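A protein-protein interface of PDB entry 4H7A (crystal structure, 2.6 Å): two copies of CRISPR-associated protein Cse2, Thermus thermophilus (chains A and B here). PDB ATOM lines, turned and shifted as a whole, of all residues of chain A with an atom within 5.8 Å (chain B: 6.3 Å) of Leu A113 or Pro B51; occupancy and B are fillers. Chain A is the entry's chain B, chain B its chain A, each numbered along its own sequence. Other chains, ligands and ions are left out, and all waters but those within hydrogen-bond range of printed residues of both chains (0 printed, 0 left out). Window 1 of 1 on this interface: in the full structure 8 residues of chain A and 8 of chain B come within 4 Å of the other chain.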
ATOM      1  N   VAL A 108      -2.390 -18.397 -22.399  1.00  0.00           N
ATOM      2  CA  VAL A 108      -1.543 -18.163 -21.250  1.00  0.00           C
ATOM      3  C   VAL A 108      -0.713 -16.934 -21.488  1.00  0.00           C
ATOM      4  O   VAL A 108      -0.592 -16.116 -20.606  1.00  0.00           O
ATOM      5  CB  VAL A 108      -0.604 -19.349 -20.985  1.00  0.00           C
ATOM      6  CG1 VAL A 108       0.687 -18.875 -20.403  1.00  0.00           C
ATOM      7  CG2 VAL A 108      -1.243 -20.337 -20.055  1.00  0.00           C
ATOM      8  N   GLU A 109      -0.164 -16.790 -22.691  1.00  0.00           N
ATOM      9  CA  GLU A 109       0.700 -15.657 -22.996  1.00  0.00           C
ATOM     10  C   GLU A 109       0.003 -14.338 -22.761  1.00  0.00           C
ATOM     11  O   GLU A 109       0.614 -13.385 -22.341  1.00  0.00           O
ATOM     12  CB  GLU A 109       1.274 -15.719 -24.399  1.00  0.00           C
ATOM     13  CG  GLU A 109       2.148 -14.507 -24.686  1.00  0.00           C
ATOM     14  CD  GLU A 109       2.904 -14.569 -25.999  1.00  0.00           C
ATOM     15  OE1 GLU A 109       3.927 -13.888 -26.102  1.00  0.00           O
ATOM     16  OE2 GLU A 109       2.499 -15.274 -26.926  1.00  0.00           O
ATOM     17  N   LYS A 110      -1.292 -14.295 -23.009  1.00  0.00           N
ATOM     18  CA  LYS A 110      -2.064 -13.128 -22.614  1.00  0.00           C
ATOM     19  C   LYS A 110      -2.091 -12.911 -21.107  1.00  0.00           C
ATOM     20  O   LYS A 110      -1.951 -11.786 -20.661  1.00  0.00           O
ATOM     21  CB  LYS A 110      -3.481 -13.203 -23.156  1.00  0.00           C
ATOM     22  CG  LYS A 110      -4.123 -11.835 -23.314  1.00  0.00           C
ATOM     23  CD  LYS A 110      -5.277 -11.861 -24.307  1.00  0.00           C
ATOM     24  CE  LYS A 110      -4.821 -12.246 -25.716  1.00  0.00           C
ATOM     25  NZ  LYS A 110      -5.245 -13.650 -26.059  1.00  0.00           N
ATOM     26  N   ARG A 111      -2.297 -13.986 -20.340  1.00  0.00           N
ATOM     27  CA  ARG A 111      -2.295 -13.920 -18.865  1.00  0.00           C
ATOM     28  C   ARG A 111      -0.988 -13.375 -18.329  1.00  0.00           C
ATOM     29  O   ARG A 111      -0.978 -12.523 -17.468  1.00  0.00           O
ATOM     30  CB  ARG A 111      -2.547 -15.298 -18.245  1.00  0.00           C
ATOM     31  CG  ARG A 111      -3.840 -15.425 -17.442  1.00  0.00           C
ATOM     32  CD  ARG A 111      -3.985 -16.801 -16.797  1.00  0.00           C
ATOM     33  NE  ARG A 111      -5.323 -17.404 -16.938  1.00  0.00           N
ATOM     34  CZ  ARG A 111      -5.700 -18.251 -17.922  1.00  0.00           C
ATOM     35  NH1 ARG A 111      -4.859 -18.625 -18.908  1.00  0.00           N
ATOM     36  NH2 ARG A 111      -6.942 -18.736 -17.926  1.00  0.00           N
ATOM     37  N   PHE A 112       0.116 -13.881 -18.856  1.00  0.00           N
ATOM     38  CA  PHE A 112       1.428 -13.436 -18.468  1.00  0.00           C
ATOM     39  C   PHE A 112       1.673 -11.945 -18.738  1.00  0.00           C
ATOM     40  O   PHE A 112       2.229 -11.236 -17.917  1.00  0.00           O
ATOM     41  CB  PHE A 112       2.474 -14.272 -19.190  1.00  0.00           C
ATOM     42  CG  PHE A 112       3.872 -13.830 -18.926  1.00  0.00           C
ATOM     43  CD1 PHE A 112       4.354 -13.810 -17.628  1.00  0.00           C
ATOM     44  CD2 PHE A 112       4.701 -13.436 -19.957  1.00  0.00           C
ATOM     45  CE1 PHE A 112       5.620 -13.400 -17.376  1.00  0.00           C
ATOM     46  CE2 PHE A 112       5.963 -13.043 -19.700  1.00  0.00           C
ATOM     47  CZ  PHE A 112       6.426 -13.020 -18.414  1.00  0.00           C
ATOM     48  N   LEU A 113       1.299 -11.476 -19.907  1.00  0.00           N
ATOM     49  CA  LEU A 113       1.457 -10.066 -20.217  1.00  0.00           C
ATOM     50  C   LEU A 113       0.548  -9.224 -19.328  1.00  0.00           C
ATOM     51  O   LEU A 113       0.906  -8.158 -18.845  1.00  0.00           O
ATOM     52  CB  LEU A 113       1.224  -9.821 -21.697  1.00  0.00           C
ATOM     53  CG  LEU A 113       2.300 -10.520 -22.525  1.00  0.00           C
ATOM     54  CD1 LEU A 113       2.070 -10.487 -24.024  1.00  0.00           C
ATOM     55  CD2 LEU A 113       3.638  -9.963 -22.191  1.00  0.00           C
ATOM     56  N   ALA A 114      -0.639  -9.737 -19.106  1.00  0.00           N
ATOM     57  CA  ALA A 114      -1.626  -9.018 -18.372  1.00  0.00           C
ATOM     58  C   ALA A 114      -1.117  -8.858 -16.955  1.00  0.00           C
ATOM     59  O   ALA A 114      -1.469  -7.930 -16.252  1.00  0.00           O
ATOM     60  CB  ALA A 114      -2.871  -9.788 -18.400  1.00  0.00           C
ATOM     61  N   LEU A 115      -0.273  -9.786 -16.552  1.00  0.00           N
ATOM     62  CA  LEU A 115       0.392  -9.723 -15.278  1.00  0.00           C
ATOM     63  C   LEU A 115       1.382  -8.581 -15.215  1.00  0.00           C
ATOM     64  O   LEU A 115       1.461  -7.897 -14.215  1.00  0.00           O
ATOM     65  CB  LEU A 115       1.101 -11.040 -15.027  1.00  0.00           C
ATOM     66  CG  LEU A 115       1.487 -11.367 -13.596  1.00  0.00           C
ATOM     67  CD1 LEU A 115       0.387 -11.046 -12.648  1.00  0.00           C
ATOM     68  CD2 LEU A 115       1.736 -12.813 -13.564  1.00  0.00           C
ATOM     69  N   LEU A 116       2.113  -8.368 -16.305  1.00  0.00           N
ATOM     70  CA  LEU A 116       3.143  -7.340 -16.339  1.00  0.00           C
ATOM     71  C   LEU A 116       2.575  -5.941 -16.316  1.00  0.00           C
ATOM     72  O   LEU A 116       3.159  -5.041 -15.740  1.00  0.00           O
ATOM     73  CB  LEU A 116       4.095  -7.564 -17.494  1.00  0.00           C
ATOM     74  CG  LEU A 116       4.631  -8.979 -17.481  1.00  0.00           C
ATOM     75  CD1 LEU A 116       5.246  -9.341 -18.760  1.00  0.00           C
ATOM     76  CD2 LEU A 116       5.636  -9.175 -16.413  1.00  0.00           C
ATOM     77  N   GLU A 117       1.404  -5.784 -16.898  1.00  0.00           N
ATOM     78  CA  GLU A 117       0.773  -4.469 -16.967  1.00  0.00           C
ATOM     79  C   GLU A 117      -0.153  -4.173 -15.847  1.00  0.00           C
ATOM     80  O   GLU A 117      -0.825  -3.183 -15.859  1.00  0.00           O
ATOM     81  CB  GLU A 117       0.010  -4.288 -18.247  1.00  0.00           C
ATOM     82  CG  GLU A 117      -0.003  -5.503 -19.077  1.00  0.00           C
ATOM     83  CD  GLU A 117      -0.894  -5.340 -20.259  1.00  0.00           C
ATOM     84  OE1 GLU A 117      -2.091  -5.610 -20.104  1.00  0.00           O
ATOM     85  OE2 GLU A 117      -0.415  -4.926 -21.334  1.00  0.00           O
ATOM     86  N   ALA A 118      -0.202  -5.057 -14.883  1.00  0.00           N
ATOM     87  CA  ALA A 118      -1.079  -4.868 -13.771  1.00  0.00           C
ATOM     88  C   ALA A 118      -0.589  -3.721 -12.895  1.00  0.00           C
ATOM     89  O   ALA A 118       0.604  -3.565 -12.667  1.00  0.00           O
ATOM     90  CB  ALA A 118      -1.149  -6.135 -12.991  1.00  0.00           C
ATOM     91  N   ARG A 155      10.842  -0.714 -14.521  1.00  0.00           N
ATOM     92  CA  ARG A 155      10.167  -1.903 -14.918  1.00  0.00           C
ATOM     93  C   ARG A 155      11.154  -3.044 -15.238  1.00  0.00           C
ATOM     94  O   ARG A 155      10.923  -3.857 -16.127  1.00  0.00           O
ATOM     95  CB  ARG A 155       9.256  -1.598 -16.103  1.00  0.00           C
ATOM     96  CG  ARG A 155       7.974  -0.880 -15.728  1.00  0.00           C
ATOM     97  CD  ARG A 155       6.827  -1.362 -16.593  1.00  0.00           C
ATOM     98  NE  ARG A 155       5.736  -1.998 -15.822  1.00  0.00           N
ATOM     99  CZ  ARG A 155       5.262  -1.540 -14.654  1.00  0.00           C
ATOM    100  NH1 ARG A 155       4.275  -2.205 -14.056  1.00  0.00           N
ATOM    101  NH2 ARG A 155       5.762  -0.418 -14.080  1.00  0.00           N
ATOM    102  N   TYR A 166      10.095 -16.018 -21.984  1.00  0.00           N
ATOM    103  CA  TYR A 166      10.437 -16.227 -23.392  1.00  0.00           C
ATOM    104  C   TYR A 166      11.734 -16.945 -23.518  1.00  0.00           C
ATOM    105  O   TYR A 166      12.045 -17.477 -24.553  1.00  0.00           O
ATOM    106  CB  TYR A 166      10.501 -14.921 -24.145  1.00  0.00           C
ATOM    107  CG  TYR A 166       9.147 -14.327 -24.372  1.00  0.00           C
ATOM    108  CD1 TYR A 166       8.319 -14.825 -25.341  1.00  0.00           C
ATOM    109  CD2 TYR A 166       8.687 -13.283 -23.602  1.00  0.00           C
ATOM    110  CE1 TYR A 166       7.094 -14.310 -25.538  1.00  0.00           C
ATOM    111  CE2 TYR A 166       7.459 -12.762 -23.798  1.00  0.00           C
ATOM    112  CZ  TYR A 166       6.671 -13.284 -24.761  1.00  0.00           C
ATOM    113  OH  TYR A 166       5.434 -12.766 -24.943  1.00  0.00           O
ATOM    114  N   GLY B  48      10.935  -1.079 -23.822  1.00  0.00           N
ATOM    115  CA  GLY B  48      10.973  -2.329 -23.086  1.00  0.00           C
ATOM    116  C   GLY B  48      10.034  -2.398 -21.901  1.00  0.00           C
ATOM    117  O   GLY B  48       9.891  -3.412 -21.304  1.00  0.00           O
ATOM    118  N   ALA B  49       9.397  -1.307 -21.562  1.00  0.00           N
ATOM    119  CA  ALA B  49       8.537  -1.287 -20.406  1.00  0.00           C
ATOM    120  C   ALA B  49       7.088  -1.443 -20.828  1.00  0.00           C
ATOM    121  O   ALA B  49       6.186  -1.278 -20.035  1.00  0.00           O
ATOM    122  CB  ALA B  49       8.715  -0.004 -19.673  1.00  0.00           C
ATOM    123  N   TYR B  50       6.868  -1.748 -22.087  1.00  0.00           N
ATOM    124  CA  TYR B  50       5.518  -1.916 -22.575  1.00  0.00           C
ATOM    125  C   TYR B  50       5.332  -3.367 -22.971  1.00  0.00           C
ATOM    126  O   TYR B  50       5.975  -3.852 -23.876  1.00  0.00           O
ATOM    127  CB  TYR B  50       5.253  -0.949 -23.737  1.00  0.00           C
ATOM    128  CG  TYR B  50       3.874  -0.989 -24.258  1.00  0.00           C
ATOM    129  CD1 TYR B  50       2.788  -0.468 -23.522  1.00  0.00           C
ATOM    130  CD2 TYR B  50       3.606  -1.566 -25.474  1.00  0.00           C
ATOM    131  CE1 TYR B  50       1.505  -0.533 -24.000  1.00  0.00           C
ATOM    132  CE2 TYR B  50       2.319  -1.625 -25.947  1.00  0.00           C
ATOM    133  CZ  TYR B  50       1.297  -1.113 -25.200  1.00  0.00           C
ATOM    134  OH  TYR B  50       0.047  -1.173 -25.670  1.00  0.00           O
ATOM    135  N   PRO B  51       4.472  -4.062 -22.241  1.00  0.00           N
ATOM    136  CA  PRO B  51       4.240  -5.488 -22.429  1.00  0.00           C
ATOM    137  C   PRO B  51       3.603  -5.955 -23.727  1.00  0.00           C
ATOM    138  O   PRO B  51       4.015  -6.979 -24.241  1.00  0.00           O
ATOM    139  CB  PRO B  51       3.363  -5.825 -21.254  1.00  0.00           C
ATOM    140  CG  PRO B  51       3.834  -4.938 -20.225  1.00  0.00           C
ATOM    141  CD  PRO B  51       4.037  -3.644 -20.901  1.00  0.00           C
ATOM    142  N   ARG B  52       2.615  -5.226 -24.245  1.00  0.00           N
ATOM    143  CA  ARG B  52       1.944  -5.622 -25.466  1.00  0.00           C
ATOM    144  C   ARG B  52       2.855  -5.679 -26.677  1.00  0.00           C
ATOM    145  O   ARG B  52       2.539  -6.356 -27.628  1.00  0.00           O
ATOM    146  CB  ARG B  52       0.755  -4.757 -25.737  1.00  0.00           C
ATOM    147  CG  ARG B  52      -0.412  -5.102 -24.856  1.00  0.00           C
ATOM    148  CD  ARG B  52      -1.506  -4.056 -24.923  1.00  0.00           C
ATOM    149  NE  ARG B  52      -2.745  -4.595 -25.477  1.00  0.00           N
ATOM    150  CZ  ARG B  52      -2.953  -4.855 -26.772  1.00  0.00           C
ATOM    151  NH1 ARG B  52      -2.000  -4.637 -27.688  1.00  0.00           N
ATOM    152  NH2 ARG B  52      -4.120  -5.356 -27.150  1.00  0.00           N
ATOM    153  N   ALA B  53       3.997  -5.001 -26.619  1.00  0.00           N
ATOM    154  CA  ALA B  53       4.998  -5.048 -27.682  1.00  0.00           C
ATOM    155  C   ALA B  53       5.943  -6.215 -27.519  1.00  0.00           C
ATOM    156  O   ALA B  53       6.729  -6.493 -28.398  1.00  0.00           O
ATOM    157  CB  ALA B  53       5.801  -3.774 -27.717  1.00  0.00           C
ATOM    158  N   MET B  54       5.862  -6.883 -26.383  1.00  0.00           N
ATOM    159  CA  MET B  54       6.809  -7.939 -26.044  1.00  0.00           C
ATOM    160  C   MET B  54       6.815  -9.173 -26.944  1.00  0.00           C
ATOM    161  O   MET B  54       7.854  -9.699 -27.291  1.00  0.00           O
ATOM    162  CB  MET B  54       6.620  -8.350 -24.583  1.00  0.00           C
ATOM    163  CG  MET B  54       7.549  -7.648 -23.651  1.00  0.00           C
ATOM    164  SD  MET B  54       7.084  -7.735 -21.954  1.00  0.00           S
ATOM    165  CE  MET B  54       8.264  -6.645 -21.252  1.00  0.00           C
ATOM    166  N   PRO B  55       5.651  -9.636 -27.323  1.00  0.00           N
ATOM    167  CA  PRO B  55       5.536 -10.885 -28.050  1.00  0.00           C
ATOM    168  C   PRO B  55       6.265 -10.817 -29.369  1.00  0.00           C
ATOM    169  O   PRO B  55       6.750 -11.803 -29.875  1.00  0.00           O
ATOM    170  CB  PRO B  55       4.058 -10.966 -28.324  1.00  0.00           C
ATOM    171  CG  PRO B  55       3.443 -10.180 -27.338  1.00  0.00           C
ATOM    172  CD  PRO B  55       4.344  -9.096 -26.959  1.00  0.00           C
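The guanidinium group (NH1) of Arg A155 sits at hydrogen-bond distance from the backbone carbonyl oxygen (O) of Leu A116, at 3.5 Å.
No position is printed for both chains.
Of the 8 pairs that touch across the chains among the printed residues, none has its exchanged pair printed and touching as well.
OE1 of Glu A109 touches CB of Pro B55, 3.7 Å away.
CD2 of Leu A113 touches O of Pro B51, at 3.6 Å.
Leu A113 touches Pro B55 (CD1 to CG, 3.6 Å).
Leu A116 touches Pro B51 (CB to CG, 3.8 Å).
Pro B51 touches Glu A117 (CB to OE2, 3.9 Å).
Arg B52 touches Glu A117 (CG to OE2, 3.5 Å).
Ala B49 touches Arg A155 (O to CD, 3.5 Å).
OH of Tyr A166 touches CA of Pro B55, at 3.6 Å.
Printed residues of chain B that touch a printed residue of chain A: Ala B49, Pro B51, Arg B52 and Pro B55.
Hydrophobic or aromatic side chains of chain B that line the printed part of chain A: Ala B49, Pro B51 and Pro B55.
Hydrophobic or aromatic side chains of chain A that line the printed part of chain B: Leu A113, Leu A116 and Tyr A166.
Along chain A the printed residues that touch a printed residue of chain B span positions 109 to 166.
Among the printed residues, no Asp or Glu carboxylate lies within 4 Å of a Lys or Arg side-chain nitrogen of the other chain.
Of chain B, only Pro B51 and Pro B55 come within 4 Å of Leu A113.
Pro B51 touches just these residues of chain A: Leu A113, Leu A116 and Glu A117.
Printed residues of chain A within 4 Å of Ala B49: Arg A155.
Of the printed residues of chain B, Glu A109 touches Pro B55 (3.7 Å).
Of the printed residues of chain B, Leu A116 touches Pro B51 (3.8 Å).
Of the printed residues of chain B, Tyr A166 touches Pro B55 (3.6 Å).
Leu A115 touches none of the printed residues of chain B.
Ala B53 touches none of the printed residues of chain A.
The nearest residue of chain A that does not touch Pro B51 is Arg A155 (5.6 Å).
The nearest printed residue of chain B that does not touch Leu A116 is Met B54 (4.02 Å).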
